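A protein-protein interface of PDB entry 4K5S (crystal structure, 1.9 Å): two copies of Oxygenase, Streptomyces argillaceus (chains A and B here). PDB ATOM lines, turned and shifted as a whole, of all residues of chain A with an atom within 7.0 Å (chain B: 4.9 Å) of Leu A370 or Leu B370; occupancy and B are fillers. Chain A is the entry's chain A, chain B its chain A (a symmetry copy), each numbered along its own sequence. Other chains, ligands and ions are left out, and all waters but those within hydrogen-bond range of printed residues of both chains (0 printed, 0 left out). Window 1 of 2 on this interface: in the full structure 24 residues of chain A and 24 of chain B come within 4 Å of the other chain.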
ATOM      1  N   ILE A  91       5.938   5.360   6.876  1.00  0.00           N
ATOM      2  CA  ILE A  91       7.153   5.804   6.228  1.00  0.00           C
ATOM      3  C   ILE A  91       8.333   5.064   6.858  1.00  0.00           C
ATOM      4  O   ILE A  91       8.508   5.102   8.076  1.00  0.00           O
ATOM      5  CB  ILE A  91       7.322   7.315   6.369  1.00  0.00           C
ATOM      6  CG1 ILE A  91       6.114   8.020   5.740  1.00  0.00           C
ATOM      7  CG2 ILE A  91       8.623   7.754   5.697  1.00  0.00           C
ATOM      8  CD1 ILE A  91       6.130   9.527   5.885  1.00  0.00           C
ATOM      9  N   LEU A 351      -4.882  13.012  19.305  1.00  0.00           N
ATOM     10  CA  LEU A 351      -4.720  13.884  18.148  1.00  0.00           C
ATOM     11  C   LEU A 351      -3.648  13.370  17.189  1.00  0.00           C
ATOM     12  O   LEU A 351      -3.804  13.466  15.972  1.00  0.00           O
ATOM     13  CB  LEU A 351      -4.414  15.314  18.581  1.00  0.00           C
ATOM     14  CG  LEU A 351      -5.556  16.056  19.283  1.00  0.00           C
ATOM     15  CD1 LEU A 351      -5.020  17.234  20.099  1.00  0.00           C
ATOM     16  CD2 LEU A 351      -6.649  16.498  18.294  1.00  0.00           C
ATOM     17  N   ARG A 354      -4.953  10.341  15.040  1.00  0.00           N
ATOM     18  CA  ARG A 354      -5.820  10.884  13.999  1.00  0.00           C
ATOM     19  C   ARG A 354      -4.980  11.519  12.877  1.00  0.00           C
ATOM     20  O   ARG A 354      -5.235  11.282  11.693  1.00  0.00           O
ATOM     21  CB  ARG A 354      -6.818  11.900  14.596  1.00  0.00           C
ATOM     22  CG  ARG A 354      -7.805  11.289  15.625  1.00  0.00           C
ATOM     23  CD  ARG A 354      -8.589  12.356  16.426  1.00  0.00           C
ATOM     24  NE  ARG A 354      -9.452  13.160  15.560  1.00  0.00           N
ATOM     25  CZ  ARG A 354     -10.056  14.284  15.928  1.00  0.00           C
ATOM     26  NH1 ARG A 354     -10.809  14.941  15.052  1.00  0.00           N
ATOM     27  NH2 ARG A 354      -9.912  14.757  17.158  1.00  0.00           N
ATOM     28  N   ALA A 355      -3.967  12.300  13.253  1.00  0.00           N
ATOM     29  CA  ALA A 355      -3.085  12.949  12.282  1.00  0.00           C
ATOM     30  C   ALA A 355      -2.344  11.935  11.409  1.00  0.00           C
ATOM     31  O   ALA A 355      -2.138  12.160  10.211  1.00  0.00           O
ATOM     32  CB  ALA A 355      -2.087  13.862  12.992  1.00  0.00           C
ATOM     33  N   GLN A 356      -1.944  10.820  12.009  1.00  0.00           N
ATOM     34  CA  GLN A 356      -1.193   9.805  11.276  1.00  0.00           C
ATOM     35  C   GLN A 356      -2.092   9.080  10.284  1.00  0.00           C
ATOM     36  O   GLN A 356      -1.659   8.704   9.197  1.00  0.00           O
ATOM     37  CB  GLN A 356      -0.536   8.810  12.229  1.00  0.00           C
ATOM     38  CG  GLN A 356       0.547   9.416  13.113  1.00  0.00           C
ATOM     39  CD  GLN A 356       1.202   8.375  14.012  1.00  0.00           C
ATOM     40  OE1 GLN A 356       1.043   8.399  15.238  1.00  0.00           O
ATOM     41  NE2 GLN A 356       1.926   7.446  13.404  1.00  0.00           N
ATOM     42  N   ALA A 358      -4.431  10.545   8.706  1.00  0.00           N
ATOM     43  CA  ALA A 358      -4.466  11.470   7.573  1.00  0.00           C
ATOM     44  C   ALA A 358      -3.231  11.248   6.702  1.00  0.00           C
ATOM     45  O   ALA A 358      -3.326  11.211   5.481  1.00  0.00           O
ATOM     46  CB  ALA A 358      -4.518  12.917   8.051  1.00  0.00           C
ATOM     47  N   LEU A 359      -2.076  11.079   7.344  1.00  0.00           N
ATOM     48  CA  LEU A 359      -0.823  10.847   6.621  1.00  0.00           C
ATOM     49  C   LEU A 359      -0.755   9.511   5.883  1.00  0.00           C
ATOM     50  O   LEU A 359       0.056   9.354   4.974  1.00  0.00           O
ATOM     51  CB  LEU A 359       0.377  10.961   7.554  1.00  0.00           C
ATOM     52  CG  LEU A 359       0.778  12.375   7.948  1.00  0.00           C
ATOM     53  CD1 LEU A 359       1.883  12.302   8.989  1.00  0.00           C
ATOM     54  CD2 LEU A 359       1.226  13.157   6.723  1.00  0.00           C
ATOM     55  N   GLN A 365      -3.713  11.021  -5.360  1.00  0.00           N
ATOM     56  CA  GLN A 365      -3.866  12.392  -5.836  1.00  0.00           C
ATOM     57  C   GLN A 365      -3.121  13.432  -4.994  1.00  0.00           C
ATOM     58  O   GLN A 365      -2.360  14.236  -5.527  1.00  0.00           O
ATOM     59  CB  GLN A 365      -5.346  12.754  -5.892  1.00  0.00           C
ATOM     60  CG  GLN A 365      -5.796  13.177  -7.245  1.00  0.00           C
ATOM     61  CD  GLN A 365      -5.310  12.234  -8.324  1.00  0.00           C
ATOM     62  OE1 GLN A 365      -4.902  12.669  -9.400  1.00  0.00           O
ATOM     63  NE2 GLN A 365      -5.350  10.931  -8.043  1.00  0.00           N
ATOM     64  N   HIS A 366      -3.349  13.417  -3.683  1.00  0.00           N
ATOM     65  CA  HIS A 366      -2.824  14.459  -2.805  1.00  0.00           C
ATOM     66  C   HIS A 366      -1.942  13.911  -1.681  1.00  0.00           C
ATOM     67  O   HIS A 366      -0.869  14.446  -1.416  1.00  0.00           O
ATOM     68  CB  HIS A 366      -3.971  15.269  -2.194  1.00  0.00           C
ATOM     69  CG  HIS A 366      -4.919  15.830  -3.203  1.00  0.00           C
ATOM     70  ND1 HIS A 366      -6.287  15.759  -3.054  1.00  0.00           N
ATOM     71  CD2 HIS A 366      -4.702  16.465  -4.380  1.00  0.00           C
ATOM     72  CE1 HIS A 366      -6.871  16.337  -4.089  1.00  0.00           C
ATOM     73  NE2 HIS A 366      -5.931  16.770  -4.910  1.00  0.00           N
ATOM     74  N   THR A 367      -2.399  12.849  -1.021  1.00  0.00           N
ATOM     75  CA  THR A 367      -1.710  12.339   0.157  1.00  0.00           C
ATOM     76  C   THR A 367      -0.332  11.756  -0.197  1.00  0.00           C
ATOM     77  O   THR A 367       0.639  11.958   0.528  1.00  0.00           O
ATOM     78  CB  THR A 367      -2.609  11.337   0.931  1.00  0.00           C
ATOM     79  OG1 THR A 367      -3.865  11.964   1.229  1.00  0.00           O
ATOM     80  CG2 THR A 367      -1.968  10.900   2.242  1.00  0.00           C
ATOM     81  N   THR A 368      -0.229  11.059  -1.328  1.00  0.00           N
ATOM     82  CA  THR A 368       1.072  10.554  -1.753  1.00  0.00           C
ATOM     83  C   THR A 368       2.118  11.682  -1.855  1.00  0.00           C
ATOM     84  O   THR A 368       3.189  11.586  -1.270  1.00  0.00           O
ATOM     85  CB  THR A 368       0.978   9.689  -3.042  1.00  0.00           C
ATOM     86  OG1 THR A 368       0.296   8.460  -2.736  1.00  0.00           O
ATOM     87  CG2 THR A 368       2.374   9.361  -3.580  1.00  0.00           C
ATOM     88  N   PRO A 369       1.803  12.770  -2.576  1.00  0.00           N
ATOM     89  CA  PRO A 369       2.758  13.893  -2.584  1.00  0.00           C
ATOM     90  C   PRO A 369       3.060  14.468  -1.191  1.00  0.00           C
ATOM     91  O   PRO A 369       4.228  14.723  -0.879  1.00  0.00           O
ATOM     92  CB  PRO A 369       2.077  14.923  -3.479  1.00  0.00           C
ATOM     93  CG  PRO A 369       1.265  14.074  -4.450  1.00  0.00           C
ATOM     94  CD  PRO A 369       0.767  12.908  -3.614  1.00  0.00           C
ATOM     95  N   LEU A 370       2.047  14.656  -0.353  1.00  0.00           N
ATOM     96  CA  LEU A 370       2.314  15.097   1.012  1.00  0.00           C
ATOM     97  C   LEU A 370       3.280  14.159   1.731  1.00  0.00           C
ATOM     98  O   LEU A 370       4.211  14.605   2.403  1.00  0.00           O
ATOM     99  CB  LEU A 370       1.016  15.228   1.808  1.00  0.00           C
ATOM    100  CG  LEU A 370       1.157  15.587   3.300  1.00  0.00           C
ATOM    101  CD1 LEU A 370       1.841  16.936   3.512  1.00  0.00           C
ATOM    102  CD2 LEU A 370      -0.214  15.593   3.962  1.00  0.00           C
ATOM    103  N   ARG A 371       3.053  12.856   1.621  1.00  0.00           N
ATOM    104  CA  ARG A 371       3.945  11.899   2.271  1.00  0.00           C
ATOM    105  C   ARG A 371       5.404  12.117   1.833  1.00  0.00           C
ATOM    106  O   ARG A 371       6.325  12.003   2.635  1.00  0.00           O
ATOM    107  CB  ARG A 371       3.481  10.455   2.018  1.00  0.00           C
ATOM    108  CG  ARG A 371       2.177  10.102   2.731  1.00  0.00           C
ATOM    109  CD  ARG A 371       1.537   8.817   2.203  1.00  0.00           C
ATOM    110  NE  ARG A 371       2.427   7.669   2.353  1.00  0.00           N
ATOM    111  CZ  ARG A 371       2.679   7.058   3.507  1.00  0.00           C
ATOM    112  NH1 ARG A 371       2.114   7.476   4.636  1.00  0.00           N
ATOM    113  NH2 ARG A 371       3.513   6.030   3.526  1.00  0.00           N
ATOM    114  N   GLY A 372       5.601  12.456   0.566  1.00  0.00           N
ATOM    115  CA  GLY A 372       6.931  12.771   0.076  1.00  0.00           C
ATOM    116  C   GLY A 372       7.616  13.898   0.837  1.00  0.00           C
ATOM    117  O   GLY A 372       8.783  13.805   1.182  1.00  0.00           O
ATOM    118  N   PHE A 373       6.906  14.986   1.097  1.00  0.00           N
ATOM    119  CA  PHE A 373       7.521  16.088   1.828  1.00  0.00           C
ATOM    120  C   PHE A 373       7.736  15.749   3.308  1.00  0.00           C
ATOM    121  O   PHE A 373       8.735  16.167   3.910  1.00  0.00           O
ATOM    122  CB  PHE A 373       6.697  17.369   1.675  1.00  0.00           C
ATOM    123  CG  PHE A 373       6.668  17.891   0.273  1.00  0.00           C
ATOM    124  CD1 PHE A 373       7.755  18.588  -0.240  1.00  0.00           C
ATOM    125  CD2 PHE A 373       5.570  17.658  -0.544  1.00  0.00           C
ATOM    126  CE1 PHE A 373       7.736  19.065  -1.543  1.00  0.00           C
ATOM    127  CE2 PHE A 373       5.541  18.129  -1.844  1.00  0.00           C
ATOM    128  CZ  PHE A 373       6.631  18.832  -2.347  1.00  0.00           C
ATOM    129  N   VAL A 374       6.800  15.005   3.893  1.00  0.00           N
ATOM    130  CA  VAL A 374       6.940  14.578   5.285  1.00  0.00           C
ATOM    131  C   VAL A 374       8.178  13.702   5.420  1.00  0.00           C
ATOM    132  O   VAL A 374       8.948  13.835   6.372  1.00  0.00           O
ATOM    133  CB  VAL A 374       5.720  13.785   5.774  1.00  0.00           C
ATOM    134  CG1 VAL A 374       5.967  13.256   7.177  1.00  0.00           C
ATOM    135  CG2 VAL A 374       4.466  14.657   5.739  1.00  0.00           C
ATOM    136  N   GLU A 375       8.369  12.802   4.457  1.00  0.00           N
ATOM    137  CA  GLU A 375       9.544  11.934   4.435  1.00  0.00           C
ATOM    138  C   GLU A 375      10.832  12.765   4.408  1.00  0.00           C
ATOM    139  O   GLU A 375      11.770  12.490   5.160  1.00  0.00           O
ATOM    140  CB  GLU A 375       9.484  10.972   3.238  1.00  0.00           C
ATOM    141  CG  GLU A 375      10.459   9.789   3.302  1.00  0.00           C
ATOM    142  CD  GLU A 375      11.824  10.093   2.691  1.00  0.00           C
ATOM    143  OE1 GLU A 375      12.025  11.231   2.226  1.00  0.00           O
ATOM    144  OE2 GLU A 375      12.694   9.190   2.665  1.00  0.00           O
ATOM    145  N   GLU A 376      10.873  13.784   3.550  1.00  0.00           N
ATOM    146  CA  GLU A 376      12.017  14.692   3.509  1.00  0.00           C
ATOM    147  C   GLU A 376      12.250  15.322   4.873  1.00  0.00           C
ATOM    148  O   GLU A 376      13.376  15.366   5.363  1.00  0.00           O
ATOM    149  CB  GLU A 376      11.787  15.841   2.522  1.00  0.00           C
ATOM    150  CG  GLU A 376      12.066  15.545   1.068  1.00  0.00           C
ATOM    151  CD  GLU A 376      11.827  16.766   0.181  1.00  0.00           C
ATOM    152  OE1 GLU A 376      12.091  17.899   0.640  1.00  0.00           O
ATOM    153  OE2 GLU A 376      11.347  16.592  -0.964  1.00  0.00           O
ATOM    154  N   PHE A 387       8.942  14.147  16.211  1.00  0.00           N
ATOM    155  CA  PHE A 387       8.070  12.987  16.128  1.00  0.00           C
ATOM    156  C   PHE A 387       8.572  11.829  16.980  1.00  0.00           C
ATOM    157  O   PHE A 387       7.776  11.083  17.534  1.00  0.00           O
ATOM    158  CB  PHE A 387       7.811  12.586  14.679  1.00  0.00           C
ATOM    159  CG  PHE A 387       6.909  13.551  13.955  1.00  0.00           C
ATOM    160  CD1 PHE A 387       5.618  13.786  14.411  1.00  0.00           C
ATOM    161  CD2 PHE A 387       7.356  14.240  12.837  1.00  0.00           C
ATOM    162  CE1 PHE A 387       4.771  14.686  13.748  1.00  0.00           C
ATOM    163  CE2 PHE A 387       6.526  15.138  12.174  1.00  0.00           C
ATOM    164  CZ  PHE A 387       5.231  15.362  12.626  1.00  0.00           C
ATOM    165  N   ALA B 355       0.237  18.369  -2.414  1.00  0.00           N
ATOM    166  CA  ALA B 355       0.434  18.176  -0.977  1.00  0.00           C
ATOM    167  C   ALA B 355      -0.403  19.149  -0.146  1.00  0.00           C
ATOM    168  O   ALA B 355      -0.926  18.790   0.915  1.00  0.00           O
ATOM    169  CB  ALA B 355       1.912  18.312  -0.617  1.00  0.00           C
ATOM    170  N   ALA B 358      -3.944  18.157   0.125  1.00  0.00           N
ATOM    171  CA  ALA B 358      -4.104  17.149   1.173  1.00  0.00           C
ATOM    172  C   ALA B 358      -4.220  17.845   2.528  1.00  0.00           C
ATOM    173  O   ALA B 358      -5.059  17.486   3.345  1.00  0.00           O
ATOM    174  CB  ALA B 358      -2.928  16.178   1.181  1.00  0.00           C
ATOM    175  N   LEU B 359      -3.382  18.858   2.747  1.00  0.00           N
ATOM    176  CA  LEU B 359      -3.402  19.611   4.004  1.00  0.00           C
ATOM    177  C   LEU B 359      -4.666  20.441   4.224  1.00  0.00           C
ATOM    178  O   LEU B 359      -4.962  20.816   5.356  1.00  0.00           O
ATOM    179  CB  LEU B 359      -2.184  20.521   4.115  1.00  0.00           C
ATOM    180  CG  LEU B 359      -0.872  19.832   4.462  1.00  0.00           C
ATOM    181  CD1 LEU B 359       0.254  20.850   4.385  1.00  0.00           C
ATOM    182  CD2 LEU B 359      -0.955  19.205   5.845  1.00  0.00           C
ATOM    183  N   HIS B 366      -9.502  13.389  10.578  1.00  0.00           N
ATOM    184  CA  HIS B 366      -8.058  13.181  10.552  1.00  0.00           C
ATOM    185  C   HIS B 366      -7.276  14.433  10.147  1.00  0.00           C
ATOM    186  O   HIS B 366      -6.279  14.775  10.777  1.00  0.00           O
ATOM    187  CB  HIS B 366      -7.701  12.036   9.599  1.00  0.00           C
ATOM    188  CG  HIS B 366      -8.431  10.765   9.882  1.00  0.00           C
ATOM    189  ND1 HIS B 366      -9.016  10.009   8.889  1.00  0.00           N
ATOM    190  CD2 HIS B 366      -8.682  10.116  11.045  1.00  0.00           C
ATOM    191  CE1 HIS B 366      -9.584   8.944   9.427  1.00  0.00           C
ATOM    192  NE2 HIS B 366      -9.399   8.987  10.733  1.00  0.00           N
ATOM    193  N   THR B 367      -7.730  15.110   9.094  1.00  0.00           N
ATOM    194  CA  THR B 367      -6.980  16.229   8.538  1.00  0.00           C
ATOM    195  C   THR B 367      -6.926  17.418   9.511  1.00  0.00           C
ATOM    196  O   THR B 367      -5.891  18.066   9.653  1.00  0.00           O
ATOM    197  CB  THR B 367      -7.528  16.619   7.137  1.00  0.00           C
ATOM    198  OG1 THR B 367      -7.534  15.458   6.295  1.00  0.00           O
ATOM    199  CG2 THR B 367      -6.672  17.689   6.473  1.00  0.00           C
ATOM    200  N   THR B 368      -8.026  17.693  10.211  1.00  0.00           N
ATOM    201  CA  THR B 368      -8.005  18.759  11.207  1.00  0.00           C
ATOM    202  C   THR B 368      -6.884  18.547  12.245  1.00  0.00           C
ATOM    203  O   THR B 368      -6.077  19.439  12.473  1.00  0.00           O
ATOM    204  CB  THR B 368      -9.400  18.993  11.852  1.00  0.00           C
ATOM    205  OG1 THR B 368     -10.285  19.559  10.869  1.00  0.00           O
ATOM    206  CG2 THR B 368      -9.296  19.956  13.038  1.00  0.00           C
ATOM    207  N   PRO B 369      -6.812  17.357  12.861  1.00  0.00           N
ATOM    208  CA  PRO B 369      -5.679  17.118  13.773  1.00  0.00           C
ATOM    209  C   PRO B 369      -4.300  17.254  13.106  1.00  0.00           C
ATOM    210  O   PRO B 369      -3.404  17.874  13.687  1.00  0.00           O
ATOM    211  CB  PRO B 369      -5.922  15.696  14.267  1.00  0.00           C
ATOM    212  CG  PRO B 369      -7.441  15.559  14.231  1.00  0.00           C
ATOM    213  CD  PRO B 369      -7.865  16.335  12.996  1.00  0.00           C
ATOM    214  N   LEU B 370      -4.123  16.712  11.906  1.00  0.00           N
ATOM    215  CA  LEU B 370      -2.862  16.919  11.202  1.00  0.00           C
ATOM    216  C   LEU B 370      -2.540  18.402  11.040  1.00  0.00           C
ATOM    217  O   LEU B 370      -1.407  18.830  11.260  1.00  0.00           O
ATOM    218  CB  LEU B 370      -2.880  16.230   9.837  1.00  0.00           C
ATOM    219  CG  LEU B 370      -1.647  16.453   8.939  1.00  0.00           C
ATOM    220  CD1 LEU B 370      -0.360  15.939   9.579  1.00  0.00           C
ATOM    221  CD2 LEU B 370      -1.861  15.777   7.592  1.00  0.00           C
ATOM    222  N   ARG B 371      -3.524  19.192  10.627  1.00  0.00           N
ATOM    223  CA  ARG B 371      -3.292  20.626  10.462  1.00  0.00           C
ATOM    224  C   ARG B 371      -2.757  21.252  11.762  1.00  0.00           C
ATOM    225  O   ARG B 371      -1.892  22.122  11.732  1.00  0.00           O
ATOM    226  CB  ARG B 371      -4.561  21.335   9.966  1.00  0.00           C
ATOM    227  CG  ARG B 371      -4.934  20.978   8.528  1.00  0.00           C
ATOM    228  CD  ARG B 371      -6.362  21.387   8.162  1.00  0.00           C
ATOM    229  NE  ARG B 371      -6.565  22.827   8.309  1.00  0.00           N
ATOM    230  CZ  ARG B 371      -6.097  23.743   7.467  1.00  0.00           C
ATOM    231  NH1 ARG B 371      -5.386  23.387   6.400  1.00  0.00           N
ATOM    232  NH2 ARG B 371      -6.335  25.022   7.705  1.00  0.00           N
ATOM    233  N   GLY B 372      -3.257  20.784  12.899  1.00  0.00           N
ATOM    234  CA  GLY B 372      -2.755  21.245  14.181  1.00  0.00           C
ATOM    235  C   GLY B 372      -1.257  21.043  14.364  1.00  0.00           C
ATOM    236  O   GLY B 372      -0.555  21.926  14.826  1.00  0.00           O
ATOM    237  N   PHE B 373      -0.747  19.870  14.017  1.00  0.00           N
ATOM    238  CA  PHE B 373       0.684  19.634  14.170  1.00  0.00           C
ATOM    239  C   PHE B 373       1.510  20.414  13.141  1.00  0.00           C
ATOM    240  O   PHE B 373       2.614  20.886  13.447  1.00  0.00           O
ATOM    241  CB  PHE B 373       0.999  18.137  14.103  1.00  0.00           C
ATOM    242  CG  PHE B 373       0.422  17.359  15.243  1.00  0.00           C
ATOM    243  CD1 PHE B 373       1.033  17.381  16.490  1.00  0.00           C
ATOM    244  CD2 PHE B 373      -0.749  16.631  15.079  1.00  0.00           C
ATOM    245  CE1 PHE B 373       0.496  16.668  17.552  1.00  0.00           C
ATOM    246  CE2 PHE B 373      -1.293  15.917  16.132  1.00  0.00           C
ATOM    247  CZ  PHE B 373      -0.670  15.939  17.375  1.00  0.00           C
ATOM    248  N   VAL B 374       0.985  20.539  11.924  1.00  0.00           N
ATOM    249  CA  VAL B 374       1.666  21.313  10.887  1.00  0.00           C
ATOM    250  C   VAL B 374       1.783  22.763  11.338  1.00  0.00           C
ATOM    251  O   VAL B 374       2.825  23.397  11.169  1.00  0.00           O
ATOM    252  CB  VAL B 374       0.918  21.274   9.547  1.00  0.00           C
ATOM    253  CG1 VAL B 374       1.593  22.193   8.542  1.00  0.00           C
ATOM    254  CG2 VAL B 374       0.855  19.843   9.012  1.00  0.00           C
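Among the printed residues, pairs that only touch across the chains: Arg A354 with His B366, Arg A354 with Pro B369, Leu A351 with Phe B373, Leu A351 with Pro B369, Ala A355 with Leu B370, Leu A370 with Ala B355, Ala A358 with His B366, His A366 with Ala B358, Ala A355 with Phe B373, Phe A373 with Ala B355, Leu A370 with Ala B358, Ala A358 with Leu B370, Ala A355 with His B366, His A366 with Ala B355 and Leu A370 with Leu B370.
Of the printed residues of chain B, Ala A355 touches His B366, Leu B370 and Phe B373.
Gln A356 touches none of the printed residues of chain B.
Gln A365 touches none of the printed residues of chain B.
Of the printed residues of chain B, Leu A370 touches Ala B355, Ala B358 and Leu B370.
Printed residues of chain A within 4 Å of Ala B355: His A366, Leu A370 and Phe A373.
Printed residues of chain A within 4 Å of Ala B358: His A366 and Leu A370.
Of the printed residues of chain A, His B366 touches Arg A354 (3.3 Å), Ala A355 (3.98 Å) and Ala A358 (3.6 Å).
Of the printed residues of chain A, Leu B370 touches Ala A355, Ala A358 and Leu A370.
Printed residues of chain A within 4 Å of Phe B373: Leu A351 and Ala A355.
The nearest printed residue of chain A that does not touch Ala B358 is Thr A367 (4.03 Å).
Of the 12 printed residues of chain B, 6 touch a printed residue of chain A.
Printed residues of chain B that touch a printed residue of chain A: Ala B355, Ala B358, His B366, Pro B369, Leu B370 and Phe B373.
Hydrophobic or aromatic side chains of chain B within 4 Å of the printed part of chain A: Ala B355, Ala B358, His B366, Pro B369, Leu B370 and Phe B373.
Of the 20 printed residues of chain A, 7 touch a printed residue of chain B.
Hydrophobic or aromatic side chains of chain A that line the printed part of chain B: Leu A351, Ala A355, Ala A358, His A366, Leu A370 and Phe A373.
Ala A355 touches Leu B370, and with the chains exchanged Leu A370 touches Ala B355.
Ala A355 touches Phe B373, and with the chains exchanged Phe A373 touches Ala B355.
Ala A358 touches Leu B370, and with the chains exchanged Leu A370 touches Ala B358.
Leu B370 touches its own counterpart, Leu A370.
12 positions are printed for both chains.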
